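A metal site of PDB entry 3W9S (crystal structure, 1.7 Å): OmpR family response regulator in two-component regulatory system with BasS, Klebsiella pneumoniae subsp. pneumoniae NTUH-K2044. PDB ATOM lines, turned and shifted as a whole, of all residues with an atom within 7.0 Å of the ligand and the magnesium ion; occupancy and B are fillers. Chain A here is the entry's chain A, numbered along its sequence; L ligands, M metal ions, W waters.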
ATOM      1  N   ILE A   6     -23.295  11.734  11.361  1.00  0.00           N
ATOM      2  CA  ILE A   6     -23.311  13.198  11.448  1.00  0.00           C
ATOM      3  C   ILE A   6     -23.889  13.550  12.806  1.00  0.00           C
ATOM      4  O   ILE A   6     -25.081  13.352  13.046  1.00  0.00           O
ATOM      5  CB  ILE A   6     -24.183  13.815  10.332  1.00  0.00           C
ATOM      6  CG1 ILE A   6     -23.748  13.293   8.963  1.00  0.00           C
ATOM      7  CG2 ILE A   6     -24.135  15.354  10.396  1.00  0.00           C
ATOM      8  CD1 ILE A   6     -24.743  13.630   7.835  1.00  0.00           C
ATOM      9  N   GLU A   7     -23.053  14.049  13.708  1.00  0.00           N
ATOM     10  CA  GLU A   7     -23.470  14.279  15.093  1.00  0.00           C
ATOM     11  C   GLU A   7     -22.523  15.316  15.701  1.00  0.00           C
ATOM     12  O   GLU A   7     -21.307  15.137  15.646  1.00  0.00           O
ATOM     13  CB  GLU A   7     -23.415  12.955  15.879  1.00  0.00           C
ATOM     14  CG  GLU A   7     -23.409  13.096  17.410  1.00  0.00           C
ATOM     15  CD  GLU A   7     -24.654  13.764  17.961  1.00  0.00           C
ATOM     16  OE1 GLU A   7     -25.761  13.224  17.765  1.00  0.00           O
ATOM     17  OE2 GLU A   7     -24.521  14.816  18.613  1.00  0.00           O
ATOM     18  N   ASP A   8     -23.077  16.379  16.269  1.00  0.00           N
ATOM     19  CA  ASP A   8     -22.229  17.477  16.730  1.00  0.00           C
ATOM     20  C   ASP A   8     -21.666  17.312  18.154  1.00  0.00           C
ATOM     21  O   ASP A   8     -20.690  17.965  18.514  1.00  0.00           O
ATOM     22  CB  ASP A   8     -22.905  18.852  16.558  1.00  0.00           C
ATOM     23  CG  ASP A   8     -24.129  19.027  17.427  1.00  0.00           C
ATOM     24  OD1 ASP A   8     -24.296  20.131  17.981  1.00  0.00           O
ATOM     25  OD2 ASP A   8     -24.937  18.080  17.527  1.00  0.00           O
ATOM     26  N   ASP A   9     -22.261  16.441  18.959  1.00  0.00           N
ATOM     27  CA  ASP A   9     -21.682  16.176  20.274  1.00  0.00           C
ATOM     28  C   ASP A   9     -20.493  15.251  20.126  1.00  0.00           C
ATOM     29  O   ASP A   9     -20.642  14.105  19.718  1.00  0.00           O
ATOM     30  CB  ASP A   9     -22.693  15.571  21.244  1.00  0.00           C
ATOM     31  CG  ASP A   9     -22.106  15.416  22.641  1.00  0.00           C
ATOM     32  OD1 ASP A   9     -22.052  16.431  23.369  1.00  0.00           O
ATOM     33  OD2 ASP A   9     -21.683  14.290  23.006  1.00  0.00           O
ATOM     34  N   LEU A  12     -20.380  11.844  22.146  1.00  0.00           N
ATOM     35  CA  LEU A  12     -21.313  10.882  21.557  1.00  0.00           C
ATOM     36  C   LEU A  12     -20.825  10.405  20.194  1.00  0.00           C
ATOM     37  O   LEU A  12     -20.822   9.194  19.922  1.00  0.00           O
ATOM     38  CB  LEU A  12     -22.725  11.463  21.446  1.00  0.00           C
ATOM     39  CG  LEU A  12     -23.782  10.488  20.931  1.00  0.00           C
ATOM     40  CD1 LEU A  12     -23.984   9.359  21.925  1.00  0.00           C
ATOM     41  CD2 LEU A  12     -25.110  11.203  20.671  1.00  0.00           C
ATOM     42  N   LEU A  50     -27.987  10.451  11.024  1.00  0.00           N
ATOM     43  CA  LEU A  50     -28.122  11.903  10.981  1.00  0.00           C
ATOM     44  C   LEU A  50     -28.767  12.511  12.231  1.00  0.00           C
ATOM     45  O   LEU A  50     -29.941  12.289  12.506  1.00  0.00           O
ATOM     46  CB  LEU A  50     -28.942  12.303   9.731  1.00  0.00           C
ATOM     47  CG  LEU A  50     -29.336  13.778   9.554  1.00  0.00           C
ATOM     48  CD1 LEU A  50     -28.094  14.612   9.271  1.00  0.00           C
ATOM     49  CD2 LEU A  50     -30.361  13.937   8.420  1.00  0.00           C
ATOM     50  N   ASP A  51     -27.984  13.301  12.967  1.00  0.00           N
ATOM     51  CA  ASP A  51     -28.495  14.115  14.065  1.00  0.00           C
ATOM     52  C   ASP A  51     -29.147  15.374  13.456  1.00  0.00           C
ATOM     53  O   ASP A  51     -28.763  15.841  12.384  1.00  0.00           O
ATOM     54  CB  ASP A  51     -27.308  14.486  14.972  1.00  0.00           C
ATOM     55  CG  ASP A  51     -27.701  15.375  16.143  1.00  0.00           C
ATOM     56  OD1 ASP A  51     -26.892  16.285  16.433  1.00  0.00           O
ATOM     57  OD2 ASP A  51     -28.766  15.184  16.773  1.00  0.00           O
ATOM     58  N   LEU A  52     -30.173  15.912  14.127  1.00  0.00           N
ATOM     59  CA  LEU A  52     -30.891  17.072  13.586  1.00  0.00           C
ATOM     60  C   LEU A  52     -30.376  18.415  14.117  1.00  0.00           C
ATOM     61  O   LEU A  52     -30.265  19.373  13.342  1.00  0.00           O
ATOM     62  CB  LEU A  52     -32.396  16.950  13.831  1.00  0.00           C
ATOM     63  CG  LEU A  52     -33.048  15.706  13.216  1.00  0.00           C
ATOM     64  CD1 LEU A  52     -34.563  15.787  13.375  1.00  0.00           C
ATOM     65  CD2 LEU A  52     -32.661  15.557  11.747  1.00  0.00           C
ATOM     66  N   GLY A  53     -30.082  18.499  15.413  1.00  0.00           N
ATOM     67  CA  GLY A  53     -29.540  19.714  15.981  1.00  0.00           C
ATOM     68  C   GLY A  53     -28.064  19.845  15.659  1.00  0.00           C
ATOM     69  O   GLY A  53     -27.224  19.192  16.287  1.00  0.00           O
ATOM     70  N   LEU A  54     -27.735  20.665  14.658  1.00  0.00           N
ATOM     71  CA  LEU A  54     -26.358  20.847  14.207  1.00  0.00           C
ATOM     72  C   LEU A  54     -26.066  22.338  14.152  1.00  0.00           C
ATOM     73  O   LEU A  54     -26.984  23.149  13.987  1.00  0.00           O
ATOM     74  CB  LEU A  54     -26.170  20.222  12.820  1.00  0.00           C
ATOM     75  CG  LEU A  54     -26.450  18.724  12.691  1.00  0.00           C
ATOM     76  CD1 LEU A  54     -26.438  18.305  11.217  1.00  0.00           C
ATOM     77  CD2 LEU A  54     -25.408  17.925  13.485  1.00  0.00           C
ATOM     78  N   PRO A  55     -24.785  22.715  14.286  1.00  0.00           N
ATOM     79  CA  PRO A  55     -24.406  24.130  14.402  1.00  0.00           C
ATOM     80  C   PRO A  55     -24.748  25.027  13.217  1.00  0.00           C
ATOM     81  O   PRO A  55     -25.133  26.180  13.426  1.00  0.00           O
ATOM     82  CB  PRO A  55     -22.878  24.078  14.554  1.00  0.00           C
ATOM     83  CG  PRO A  55     -22.597  22.745  15.115  1.00  0.00           C
ATOM     84  CD  PRO A  55     -23.640  21.822  14.527  1.00  0.00           C
ATOM     85  N   ILE A  77     -32.384   8.878  11.180  1.00  0.00           N
ATOM     86  CA  ILE A  77     -32.307  10.083  12.000  1.00  0.00           C
ATOM     87  C   ILE A  77     -32.179   9.655  13.465  1.00  0.00           C
ATOM     88  O   ILE A  77     -32.912   8.792  13.933  1.00  0.00           O
ATOM     89  CB  ILE A  77     -33.543  10.973  11.808  1.00  0.00           C
ATOM     90  CG1 ILE A  77     -33.446  11.735  10.484  1.00  0.00           C
ATOM     91  CG2 ILE A  77     -33.670  11.977  12.936  1.00  0.00           C
ATOM     92  CD1 ILE A  77     -34.723  12.518  10.162  1.00  0.00           C
ATOM     93  N   LEU A  78     -31.226  10.280  14.160  1.00  0.00           N
ATOM     94  CA  LEU A  78     -30.899   9.929  15.533  1.00  0.00           C
ATOM     95  C   LEU A  78     -30.835  11.241  16.318  1.00  0.00           C
ATOM     96  O   LEU A  78     -29.894  12.003  16.176  1.00  0.00           O
ATOM     97  CB  LEU A  78     -29.538   9.211  15.544  1.00  0.00           C
ATOM     98  CG  LEU A  78     -29.103   8.439  16.781  1.00  0.00           C
ATOM     99  CD1 LEU A  78     -30.037   7.251  17.014  1.00  0.00           C
ATOM    100  CD2 LEU A  78     -27.672   7.971  16.612  1.00  0.00           C
ATOM    101  N   THR A  79     -31.842  11.528  17.129  1.00  0.00           N
ATOM    102  CA  THR A  79     -32.045  12.912  17.544  1.00  0.00           C
ATOM    103  C   THR A  79     -32.759  13.067  18.876  1.00  0.00           C
ATOM    104  O   THR A  79     -33.595  12.241  19.243  1.00  0.00           O
ATOM    105  CB  THR A  79     -32.885  13.652  16.474  1.00  0.00           C
ATOM    106  OG1 THR A  79     -33.097  15.013  16.842  1.00  0.00           O
ATOM    107  CG2 THR A  79     -34.247  12.967  16.293  1.00  0.00           C
ATOM    108  N   ALA A  80     -32.457  14.162  19.577  1.00  0.00           N
ATOM    109  CA  ALA A  80     -33.190  14.551  20.782  1.00  0.00           C
ATOM    110  C   ALA A  80     -34.574  15.115  20.471  1.00  0.00           C
ATOM    111  O   ALA A  80     -35.398  15.261  21.381  1.00  0.00           O
ATOM    112  CB  ALA A  80     -32.384  15.553  21.587  1.00  0.00           C
ATOM    113  N   ARG A  81     -34.840  15.468  19.218  1.00  0.00           N
ATOM    114  CA  ARG A  81     -36.155  15.990  18.845  1.00  0.00           C
ATOM    115  C   ARG A  81     -37.185  14.868  18.855  1.00  0.00           C
ATOM    116  O   ARG A  81     -37.240  14.057  17.929  1.00  0.00           O
ATOM    117  CB  ARG A  81     -36.120  16.637  17.465  1.00  0.00           C
ATOM    118  CG  ARG A  81     -35.179  17.803  17.391  1.00  0.00           C
ATOM    119  CD  ARG A  81     -35.634  18.830  16.368  1.00  0.00           C
ATOM    120  NE  ARG A  81     -34.582  19.811  16.194  1.00  0.00           N
ATOM    121  CZ  ARG A  81     -34.053  20.136  15.023  1.00  0.00           C
ATOM    122  NH1 ARG A  81     -33.088  21.034  14.967  1.00  0.00           N
ATOM    123  NH2 ARG A  81     -34.513  19.573  13.924  1.00  0.00           N
ATOM    124  N   LYS A 101     -33.284  10.100  21.035  1.00  0.00           N
ATOM    125  CA  LYS A 101     -32.387  10.055  22.197  1.00  0.00           C
ATOM    126  C   LYS A 101     -33.166  10.276  23.479  1.00  0.00           C
ATOM    127  O   LYS A 101     -34.103  11.064  23.506  1.00  0.00           O
ATOM    128  CB  LYS A 101     -31.338  11.163  22.089  1.00  0.00           C
ATOM    129  CG  LYS A 101     -30.436  11.055  20.877  1.00  0.00           C
ATOM    130  CD  LYS A 101     -29.529  12.292  20.804  1.00  0.00           C
ATOM    131  CE  LYS A 101     -28.541  12.203  19.666  1.00  0.00           C
ATOM    132  NZ  LYS A 101     -27.768  13.493  19.599  1.00  0.00           N
HETATM  133 BE1  LIG L   1     -29.812  16.312  18.018  1.00  0.00          BE
HETATM  134  F1  LIG L   1     -28.918  17.369  18.086  1.00  0.00           F
HETATM  135  F2  LIG L   1     -30.896  16.450  17.186  1.00  0.00           F
HETATM  136  F3  LIG L   1     -29.858  15.383  19.041  1.00  0.00           F
HETATM  137 MG    MG M   1     -26.943  17.797  17.850  1.00  0.00          MG
HETATM  138  O   HOH W   1     -31.883  18.554  18.877  1.00  0.00           O
HETATM  139  O   HOH W   2     -29.205  16.775  21.440  1.00  0.00           O
HETATM  140  O   HOH W   3     -26.500  16.307  19.409  1.00  0.00           O
HETATM  141  O   HOH W   4     -27.084  19.306  19.315  1.00  0.00           O
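Hydrophobic or aromatic side chains that line the ligand: Leu 52 and Ala 80. Within 4 Å of the ligand: Asp 51, Leu 52, Gly 53, Thr 79, Ala 80 and Lys 101.
F3 of the ligand is in hydrogen-bond range of NZ of Lys 101, at 2.9 Å. F2 of the ligand sits at hydrogen-bond distance from OG1 of Thr 79 (2.7 Å). A fluorine (F2) of the ligand sits at hydrogen-bond distance from the backbone NH (N) of Leu 52. N of Ala 80 lies within hydrogen-bond range of F3 of the ligand (2.9 Å). OD2 of Asp 51 is bound to BE1 of the ligand, 2.0 Å away. The backbone NH of Gly 53 lies within hydrogen-bond range of a fluorine (F2) of the ligand, 2.8 Å away.
Water W3 lies within hydrogen-bond range of the side-chain carboxylate (OE2) of Glu 7 (2.6 Å) and the side-chain amino group (NZ) of Lys 101 (3.1 Å).
NZ of Lys 101 is in salt-bridge range of OE1 of Glu 7 (2.7 Å). OE2 of Glu 7 lies within hydrogen-bond range of N of Asp 9, 2.8 Å away. O of Thr 79 is in hydrogen-bond range of N of Lys 101, at 2.8 Å. O of Ile 6 lies within hydrogen-bond range of N of Asp 51, at 2.9 Å. NZ of Lys 101 lies close to OD2 of Asp 51, at 3.4 Å. OG1 of Thr 79 sits at hydrogen-bond distance from N of Arg 81, 3.0 Å away.
Glu 7 touches the magnesium ion (OE2 to MG, 3.9 Å). Of the 17 residues printed, 4 come within 4 Å of the magnesium ion.
The magnesium ion is bound by F1 of the ligand (2.0 Å), OD2 of Asp 8 (2.1 Å), OD1 of Asp 51 (2.1 Å), water W4 (2.1 Å), O of Gly 53 (2.1 Å) and water W3 (2.2 Å). The magnesium ion has six donor atoms within binding distance.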
